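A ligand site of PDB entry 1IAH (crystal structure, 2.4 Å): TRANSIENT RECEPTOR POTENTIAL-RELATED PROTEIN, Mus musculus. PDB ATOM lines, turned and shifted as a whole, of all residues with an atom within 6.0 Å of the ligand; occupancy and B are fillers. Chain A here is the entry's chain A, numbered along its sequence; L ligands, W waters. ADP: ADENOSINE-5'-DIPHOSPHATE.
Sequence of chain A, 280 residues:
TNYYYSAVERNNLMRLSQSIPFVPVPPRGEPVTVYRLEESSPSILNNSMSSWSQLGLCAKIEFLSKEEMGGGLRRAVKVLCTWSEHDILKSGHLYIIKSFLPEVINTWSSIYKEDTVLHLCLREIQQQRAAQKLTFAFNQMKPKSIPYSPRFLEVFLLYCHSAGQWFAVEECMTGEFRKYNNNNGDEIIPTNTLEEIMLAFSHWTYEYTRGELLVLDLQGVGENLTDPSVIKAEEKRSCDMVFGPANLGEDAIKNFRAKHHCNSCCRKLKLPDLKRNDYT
O2A of the ligand lies close to OD2 of Asp 227, 2.4 Å away.
The backbone NH (N) of Arg 74 lies within hydrogen-bond range of an oxygen (O2B) of the ligand (2.6 Å).
An oxygen (O2A) of the ligand lies within salt-bridge range of the guanidinium group of Arg 74 (3.9 Å).
The side-chain carboxylate (OE2) of Glu 170 sits at hydrogen-bond distance from a nitrogen (N6) of the ligand (2.7 Å).
N of Gly 72 is in hydrogen-bond range of O1B of the ligand (2.8 Å).
An oxygen (O2A) of the ligand is in salt-bridge range of the side-chain amino group (NZ) of Lys 98 (2.8 Å).
The backbone NH (N) of Met 173 is in hydrogen-bond range of a nitrogen (N1) of the ligand, at 3.0 Å.
The backbone NH of Leu 73 lies within hydrogen-bond range of an oxygen (O2B) of the ligand, 3.1 Å away.
A nitrogen (N6) of the ligand lies within hydrogen-bond range of the backbone carbonyl oxygen (O) of Glu 171 (3.3 Å).
OD1 of Asp 227 lies within salt-bridge range of NH2 of Arg 74.
OD1 of Asp 227 is in salt-bridge range of NZ of Lys 98 (2.8 Å).
The backbone carbonyl oxygen (O) of Asp 227 lies within hydrogen-bond range of the side-chain amide nitrogen (NE2) of Gln 219, at 3.1 Å.
The guanidinium group (NH2) of Arg 74 lies within salt-bridge range of the side-chain carboxylate (OE2) of Glu 124 (3.8 Å).
The side-chain carboxylate (OE1) of Glu 170 is in salt-bridge range of the side-chain amino group (NZ) of Lys 98 (3.3 Å).
The backbone carbonyl oxygen (O) of Glu 170 is in hydrogen-bond range of the backbone NH (N) of Ile 96 (2.7 Å).
OG1 of Thr 226 is in hydrogen-bond range of OE2 of Glu 170 (2.6 Å).
N of Ala 76 lies within hydrogen-bond range of O of Met 69.
SD of Met 69 lies close to O4' of the ligand (3.5 Å).
C of Gly 70 touches C5' of the ligand (3.8 Å).
Gly 71 touches the ligand (CA to O1B, 3.2 Å).
Ala 76 touches the ligand.
CG1 of Ile 96 touches C6 of the ligand, 3.9 Å away.
Leu 153 touches the ligand.
Cys 172 touches the ligand.
Phe 177 touches the ligand (CE2 to C4, 3.9 Å).
CG2 of Thr 226 touches N7 of the ligand (3.99 Å).
Hydrophobic or aromatic side chains that line the ligand: Met 69, Ala 76, Ile 96, Leu 153, Met 173 and Phe 177.
Within 4 Å of the ligand: Met 69, Gly 70, Gly 71, Gly 72, Leu 73, Arg 74, Ala 76, Ile 96, Lys 98, Leu 153, Glu 170, Glu 171, Cys 172, Met 173, Phe 177, Thr 226 and Asp 227.
Along chain A the residues within 4 Å of the ligand span positions 69 to 227.
The nearest printed residue that does not touch the ligand is Arg 75 (4.3 Å).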
ATOM      1  N   MET A  69       8.852  26.653 -21.760  1.00  0.00           N
ATOM      2  CA  MET A  69       9.301  25.787 -20.672  1.00  0.00           C
ATOM      3  C   MET A  69       8.555  26.055 -19.358  1.00  0.00           C
ATOM      4  O   MET A  69       8.340  27.214 -18.975  1.00  0.00           O
ATOM      5  CB  MET A  69      10.805  25.977 -20.444  1.00  0.00           C
ATOM      6  CG  MET A  69      11.673  25.455 -21.589  1.00  0.00           C
ATOM      7  SD  MET A  69      13.448  25.841 -21.437  1.00  0.00           S
ATOM      8  CE  MET A  69      13.498  27.536 -22.052  1.00  0.00           C
ATOM      9  N   GLY A  70       8.157  24.979 -18.682  1.00  0.00           N
ATOM     10  CA  GLY A  70       7.437  25.126 -17.428  1.00  0.00           C
ATOM     11  C   GLY A  70       7.828  24.137 -16.354  1.00  0.00           C
ATOM     12  O   GLY A  70       8.030  22.950 -16.628  1.00  0.00           O
ATOM     13  N   GLY A  71       7.935  24.619 -15.126  1.00  0.00           N
ATOM     14  CA  GLY A  71       8.284  23.765 -13.997  1.00  0.00           C
ATOM     15  C   GLY A  71       7.198  23.867 -12.942  1.00  0.00           C
ATOM     16  O   GLY A  71       6.058  23.471 -13.187  1.00  0.00           O
ATOM     17  N   GLY A  72       7.537  24.407 -11.769  1.00  0.00           N
ATOM     18  CA  GLY A  72       6.562  24.548 -10.712  1.00  0.00           C
ATOM     19  C   GLY A  72       5.925  25.927 -10.589  1.00  0.00           C
ATOM     20  O   GLY A  72       4.726  26.082 -10.867  1.00  0.00           O
ATOM     21  N   LEU A  73       6.720  26.927 -10.203  1.00  0.00           N
ATOM     22  CA  LEU A  73       6.225  28.297 -10.022  1.00  0.00           C
ATOM     23  C   LEU A  73       6.578  29.317 -11.104  1.00  0.00           C
ATOM     24  O   LEU A  73       6.167  30.477 -11.019  1.00  0.00           O
ATOM     25  CB  LEU A  73       6.713  28.855  -8.689  1.00  0.00           C
ATOM     26  CG  LEU A  73       7.123  27.937  -7.542  1.00  0.00           C
ATOM     27  CD1 LEU A  73       8.624  27.714  -7.577  1.00  0.00           C
ATOM     28  CD2 LEU A  73       6.743  28.586  -6.225  1.00  0.00           C
ATOM     29  N   ARG A  74       7.337  28.913 -12.114  1.00  0.00           N
ATOM     30  CA  ARG A  74       7.740  29.862 -13.144  1.00  0.00           C
ATOM     31  C   ARG A  74       7.544  29.447 -14.606  1.00  0.00           C
ATOM     32  O   ARG A  74       7.420  28.272 -14.923  1.00  0.00           O
ATOM     33  CB  ARG A  74       9.212  30.223 -12.931  1.00  0.00           C
ATOM     34  CG  ARG A  74       9.488  31.692 -12.661  1.00  0.00           C
ATOM     35  CD  ARG A  74      10.268  31.888 -11.380  1.00  0.00           C
ATOM     36  NE  ARG A  74      11.435  31.014 -11.278  1.00  0.00           N
ATOM     37  CZ  ARG A  74      12.690  31.431 -11.197  1.00  0.00           C
ATOM     38  NH1 ARG A  74      12.973  32.731 -11.195  1.00  0.00           N
ATOM     39  NH2 ARG A  74      13.683  30.549 -11.096  1.00  0.00           N
ATOM     40  N   ARG A  75       7.503  30.456 -15.463  1.00  0.00           N
ATOM     41  CA  ARG A  75       7.394  30.272 -16.907  1.00  0.00           C
ATOM     42  C   ARG A  75       8.767  30.714 -17.402  1.00  0.00           C
ATOM     43  O   ARG A  75       9.320  31.698 -16.896  1.00  0.00           O
ATOM     44  CB  ARG A  75       6.314  31.182 -17.504  1.00  0.00           C
ATOM     45  CG  ARG A  75       4.898  30.636 -17.400  1.00  0.00           C
ATOM     46  CD  ARG A  75       3.893  31.552 -18.095  1.00  0.00           C
ATOM     47  NE  ARG A  75       3.871  32.892 -17.519  1.00  0.00           N
ATOM     48  CZ  ARG A  75       4.279  33.992 -18.148  1.00  0.00           C
ATOM     49  NH1 ARG A  75       4.735  33.908 -19.394  1.00  0.00           N
ATOM     50  NH2 ARG A  75       4.231  35.175 -17.532  1.00  0.00           N
ATOM     51  N   ALA A  76       9.323  29.989 -18.366  1.00  0.00           N
ATOM     52  CA  ALA A  76      10.653  30.305 -18.889  1.00  0.00           C
ATOM     53  C   ALA A  76      10.699  30.322 -20.412  1.00  0.00           C
ATOM     54  O   ALA A  76      10.057  29.512 -21.077  1.00  0.00           O
ATOM     55  CB  ALA A  76      11.670  29.308 -18.347  1.00  0.00           C
ATOM     56  N   ILE A  96      18.104  32.065 -20.526  1.00  0.00           N
ATOM     57  CA  ILE A  96      16.754  31.659 -20.174  1.00  0.00           C
ATOM     58  C   ILE A  96      16.179  32.754 -19.275  1.00  0.00           C
ATOM     59  O   ILE A  96      16.812  33.142 -18.302  1.00  0.00           O
ATOM     60  CB  ILE A  96      16.737  30.316 -19.411  1.00  0.00           C
ATOM     61  CG1 ILE A  96      17.400  29.217 -20.235  1.00  0.00           C
ATOM     62  CG2 ILE A  96      15.298  29.931 -19.082  1.00  0.00           C
ATOM     63  CD1 ILE A  96      16.673  28.859 -21.525  1.00  0.00           C
ATOM     64  N   ILE A  97      15.005  33.258 -19.611  1.00  0.00           N
ATOM     65  CA  ILE A  97      14.392  34.307 -18.810  1.00  0.00           C
ATOM     66  C   ILE A  97      13.201  33.722 -18.084  1.00  0.00           C
ATOM     67  O   ILE A  97      12.350  33.080 -18.712  1.00  0.00           O
ATOM     68  CB  ILE A  97      13.958  35.481 -19.685  1.00  0.00           C
ATOM     69  CG1 ILE A  97      15.181  36.119 -20.320  1.00  0.00           C
ATOM     70  CG2 ILE A  97      13.189  36.498 -18.861  1.00  0.00           C
ATOM     71  CD1 ILE A  97      14.860  37.228 -21.281  1.00  0.00           C
ATOM     72  N   LYS A  98      13.116  33.947 -16.772  1.00  0.00           N
ATOM     73  CA  LYS A  98      12.024  33.401 -15.970  1.00  0.00           C
ATOM     74  C   LYS A  98      11.138  34.446 -15.285  1.00  0.00           C
ATOM     75  O   LYS A  98      11.612  35.511 -14.863  1.00  0.00           O
ATOM     76  CB  LYS A  98      12.608  32.448 -14.926  1.00  0.00           C
ATOM     77  CG  LYS A  98      13.638  31.494 -15.518  1.00  0.00           C
ATOM     78  CD  LYS A  98      14.247  30.554 -14.481  1.00  0.00           C
ATOM     79  CE  LYS A  98      15.238  29.614 -15.158  1.00  0.00           C
ATOM     80  NZ  LYS A  98      15.769  28.556 -14.258  1.00  0.00           N
ATOM     81  N   GLU A 124      14.631  35.346  -5.259  1.00  0.00           N
ATOM     82  CA  GLU A 124      14.988  34.152  -6.009  1.00  0.00           C
ATOM     83  C   GLU A 124      16.471  34.198  -6.372  1.00  0.00           C
ATOM     84  O   GLU A 124      17.210  33.234  -6.161  1.00  0.00           O
ATOM     85  CB  GLU A 124      14.158  34.073  -7.297  1.00  0.00           C
ATOM     86  CG  GLU A 124      14.205  32.716  -7.988  1.00  0.00           C
ATOM     87  CD  GLU A 124      13.754  31.590  -7.065  1.00  0.00           C
ATOM     88  OE1 GLU A 124      14.386  31.394  -6.011  1.00  0.00           O
ATOM     89  OE2 GLU A 124      12.769  30.900  -7.414  1.00  0.00           O
ATOM     90  N   LEU A 153      24.591  28.491 -11.514  1.00  0.00           N
ATOM     91  CA  LEU A 153      24.682  29.557 -12.496  1.00  0.00           C
ATOM     92  C   LEU A 153      24.398  30.876 -11.789  1.00  0.00           C
ATOM     93  O   LEU A 153      23.720  30.904 -10.766  1.00  0.00           O
ATOM     94  CB  LEU A 153      23.644  29.379 -13.594  1.00  0.00           C
ATOM     95  CG  LEU A 153      23.698  28.096 -14.426  1.00  0.00           C
ATOM     96  CD1 LEU A 153      22.484  28.099 -15.371  1.00  0.00           C
ATOM     97  CD2 LEU A 153      25.019  28.002 -15.204  1.00  0.00           C
ATOM     98  N   GLU A 170      19.424  33.980 -16.802  1.00  0.00           N
ATOM     99  CA  GLU A 170      20.631  33.192 -16.581  1.00  0.00           C
ATOM    100  C   GLU A 170      20.969  32.517 -17.890  1.00  0.00           C
ATOM    101  O   GLU A 170      20.132  32.392 -18.786  1.00  0.00           O
ATOM    102  CB  GLU A 170      20.382  32.126 -15.527  1.00  0.00           C
ATOM    103  CG  GLU A 170      19.346  31.100 -15.947  1.00  0.00           C
ATOM    104  CD  GLU A 170      18.837  30.273 -14.795  1.00  0.00           C
ATOM    105  OE1 GLU A 170      18.122  30.833 -13.937  1.00  0.00           O
ATOM    106  OE2 GLU A 170      19.126  29.059 -14.746  1.00  0.00           O
ATOM    107  N   GLU A 171      22.214  32.056 -17.982  1.00  0.00           N
ATOM    108  CA  GLU A 171      22.674  31.375 -19.182  1.00  0.00           C
ATOM    109  C   GLU A 171      21.928  30.090 -19.393  1.00  0.00           C
ATOM    110  O   GLU A 171      21.594  29.389 -18.440  1.00  0.00           O
ATOM    111  CB  GLU A 171      24.153  31.056 -19.088  1.00  0.00           C
ATOM    112  CG  GLU A 171      25.023  32.269 -18.964  1.00  0.00           C
ATOM    113  CD  GLU A 171      26.464  31.988 -19.348  1.00  0.00           C
ATOM    114  OE1 GLU A 171      26.711  31.663 -20.545  1.00  0.00           O
ATOM    115  OE2 GLU A 171      27.339  32.108 -18.470  1.00  0.00           O
ATOM    116  N   CYS A 172      21.682  29.773 -20.655  1.00  0.00           N
ATOM    117  CA  CYS A 172      20.996  28.551 -21.008  1.00  0.00           C
ATOM    118  C   CYS A 172      22.029  27.443 -21.100  1.00  0.00           C
ATOM    119  O   CYS A 172      23.063  27.581 -21.748  1.00  0.00           O
ATOM    120  CB  CYS A 172      20.283  28.715 -22.351  1.00  0.00           C
ATOM    121  SG  CYS A 172      19.387  27.260 -22.902  1.00  0.00           S
ATOM    122  N   MET A 173      21.771  26.332 -20.418  1.00  0.00           N
ATOM    123  CA  MET A 173      22.700  25.204 -20.451  1.00  0.00           C
ATOM    124  C   MET A 173      22.285  24.266 -21.577  1.00  0.00           C
ATOM    125  O   MET A 173      21.111  24.200 -21.949  1.00  0.00           O
ATOM    126  CB  MET A 173      22.684  24.448 -19.123  1.00  0.00           C
ATOM    127  CG  MET A 173      23.158  25.266 -17.938  1.00  0.00           C
ATOM    128  SD  MET A 173      23.102  24.327 -16.377  1.00  0.00           S
ATOM    129  CE  MET A 173      21.392  24.343 -16.085  1.00  0.00           C
ATOM    130  N   THR A 174      23.241  23.554 -22.129  1.00  0.00           N
ATOM    131  CA  THR A 174      22.920  22.624 -23.190  1.00  0.00           C
ATOM    132  C   THR A 174      23.188  21.221 -22.672  1.00  0.00           C
ATOM    133  O   THR A 174      24.210  20.971 -22.033  1.00  0.00           O
ATOM    134  CB  THR A 174      23.758  22.895 -24.455  1.00  0.00           C
ATOM    135  OG1 THR A 174      23.347  21.994 -25.499  1.00  0.00           O
ATOM    136  CG2 THR A 174      25.250  22.717 -24.150  1.00  0.00           C
ATOM    137  N   PHE A 177      18.827  18.090 -19.000  1.00  0.00           N
ATOM    138  CA  PHE A 177      18.571  18.711 -17.725  1.00  0.00           C
ATOM    139  C   PHE A 177      17.928  17.680 -16.802  1.00  0.00           C
ATOM    140  O   PHE A 177      16.921  17.047 -17.158  1.00  0.00           O
ATOM    141  CB  PHE A 177      17.630  19.908 -17.936  1.00  0.00           C
ATOM    142  CG  PHE A 177      17.468  20.779 -16.726  1.00  0.00           C
ATOM    143  CD1 PHE A 177      16.604  20.413 -15.695  1.00  0.00           C
ATOM    144  CD2 PHE A 177      18.158  21.993 -16.641  1.00  0.00           C
ATOM    145  CE1 PHE A 177      16.419  21.258 -14.589  1.00  0.00           C
ATOM    146  CE2 PHE A 177      17.963  22.850 -15.547  1.00  0.00           C
ATOM    147  CZ  PHE A 177      17.093  22.476 -14.520  1.00  0.00           C
ATOM    148  N   LYS A 179      16.984  16.449 -12.470  1.00  0.00           N
ATOM    149  CA  LYS A 179      16.807  16.784 -11.061  1.00  0.00           C
ATOM    150  C   LYS A 179      17.423  15.668 -10.219  1.00  0.00           C
ATOM    151  O   LYS A 179      17.027  14.514 -10.340  1.00  0.00           O
ATOM    152  CB  LYS A 179      15.316  16.911 -10.777  1.00  0.00           C
ATOM    153  CG  LYS A 179      14.965  17.714  -9.554  1.00  0.00           C
ATOM    154  CD  LYS A 179      13.536  18.225  -9.688  1.00  0.00           C
ATOM    155  CE  LYS A 179      13.248  19.379  -8.759  1.00  0.00           C
ATOM    156  NZ  LYS A 179      11.989  20.089  -9.129  1.00  0.00           N
ATOM    157  N   GLN A 219      19.358  20.556  -9.361  1.00  0.00           N
ATOM    158  CA  GLN A 219      18.997  20.229 -10.738  1.00  0.00           C
ATOM    159  C   GLN A 219      19.788  21.034 -11.759  1.00  0.00           C
ATOM    160  O   GLN A 219      20.159  22.190 -11.520  1.00  0.00           O
ATOM    161  CB  GLN A 219      17.518  20.483 -10.946  1.00  0.00           C
ATOM    162  CG  GLN A 219      17.114  21.888 -10.639  1.00  0.00           C
ATOM    163  CD  GLN A 219      15.633  22.085 -10.692  1.00  0.00           C
ATOM    164  OE1 GLN A 219      14.968  21.621 -11.622  1.00  0.00           O
ATOM    165  NE2 GLN A 219      15.079  22.786  -9.705  1.00  0.00           N
ATOM    166  N   VAL A 221      22.509  20.424 -15.521  1.00  0.00           N
ATOM    167  CA  VAL A 221      23.133  19.588 -16.519  1.00  0.00           C
ATOM    168  C   VAL A 221      24.554  19.379 -16.064  1.00  0.00           C
ATOM    169  O   VAL A 221      25.296  20.332 -15.892  1.00  0.00           O
ATOM    170  CB  VAL A 221      23.148  20.296 -17.909  1.00  0.00           C
ATOM    171  CG1 VAL A 221      23.940  19.469 -18.899  1.00  0.00           C
ATOM    172  CG2 VAL A 221      21.722  20.527 -18.403  1.00  0.00           C
ATOM    173  N   THR A 226      20.984  24.936 -11.092  1.00  0.00           N
ATOM    174  CA  THR A 226      20.172  26.138 -11.059  1.00  0.00           C
ATOM    175  C   THR A 226      18.848  25.841 -10.362  1.00  0.00           C
ATOM    176  O   THR A 226      18.505  24.675 -10.168  1.00  0.00           O
ATOM    177  CB  THR A 226      19.921  26.656 -12.483  1.00  0.00           C
ATOM    178  OG1 THR A 226      19.429  27.992 -12.434  1.00  0.00           O
ATOM    179  CG2 THR A 226      18.923  25.765 -13.199  1.00  0.00           C
ATOM    180  N   ASP A 227      18.100  26.878  -9.982  1.00  0.00           N
ATOM    181  CA  ASP A 227      16.799  26.743  -9.301  1.00  0.00           C
ATOM    182  C   ASP A 227      16.841  25.926  -8.015  1.00  0.00           C
ATOM    183  O   ASP A 227      16.033  25.033  -7.821  1.00  0.00           O
ATOM    184  CB  ASP A 227      15.756  26.080 -10.189  1.00  0.00           C
ATOM    185  CG  ASP A 227      15.458  26.869 -11.452  1.00  0.00           C
ATOM    186  OD1 ASP A 227      15.752  28.090 -11.492  1.00  0.00           O
ATOM    187  OD2 ASP A 227      14.904  26.255 -12.392  1.00  0.00           O
HETATM  188  PB  ADP L   1      10.644  26.408 -11.990  1.00  0.00           P
HETATM  189  O1B ADP L   1      10.247  24.962 -11.841  1.00  0.00           O
HETATM  190  O2B ADP L   1       9.489  27.459 -11.590  1.00  0.00           O
HETATM  191  O3B ADP L   1      11.883  26.672 -11.184  1.00  0.00           O
HETATM  192  PA  ADP L   1      12.091  27.172 -14.399  1.00  0.00           P
HETATM  193  O1A ADP L   1      11.607  28.293 -15.224  1.00  0.00           O
HETATM  194  O2A ADP L   1      13.207  27.579 -13.549  1.00  0.00           O
HETATM  195  O3A ADP L   1      10.881  26.646 -13.519  1.00  0.00           O
HETATM  196  O5' ADP L   1      12.453  25.885 -15.293  1.00  0.00           O
HETATM  197  C5' ADP L   1      11.473  25.330 -16.201  1.00  0.00           C
HETATM  198  C4' ADP L   1      12.126  24.319 -17.171  1.00  0.00           C
HETATM  199  O4' ADP L   1      12.996  24.991 -18.111  1.00  0.00           O
HETATM  200  C3' ADP L   1      12.986  23.239 -16.496  1.00  0.00           C
HETATM  201  O3' ADP L   1      12.275  22.007 -16.311  1.00  0.00           O
HETATM  202  C2' ADP L   1      14.169  23.017 -17.439  1.00  0.00           C
HETATM  203  O2' ADP L   1      13.979  21.911 -18.342  1.00  0.00           O
HETATM  204  C1' ADP L   1      14.305  24.366 -18.142  1.00  0.00           C
HETATM  205  N9  ADP L   1      15.433  25.250 -17.581  1.00  0.00           N
HETATM  206  C8  ADP L   1      15.385  26.006 -16.460  1.00  0.00           C
HETATM  207  N7  ADP L   1      16.552  26.638 -16.289  1.00  0.00           N
HETATM  208  C5  ADP L   1      17.354  26.310 -17.273  1.00  0.00           C
HETATM  209  C6  ADP L   1      18.672  26.633 -17.651  1.00  0.00           C
HETATM  210  N6  ADP L   1      19.390  27.498 -16.909  1.00  0.00           N
HETATM  211  N1  ADP L   1      19.230  26.081 -18.798  1.00  0.00           N
HETATM  212  C2  ADP L   1      18.536  25.216 -19.575  1.00  0.00           C
HETATM  213  N3  ADP L   1      17.269  24.907 -19.221  1.00  0.00           N
HETATM  214  C4  ADP L   1      16.646  25.404 -18.111  1.00  0.00           C
HETATM  215  O   HOH W   1      16.593  22.666 -20.943  1.00  0.00           O
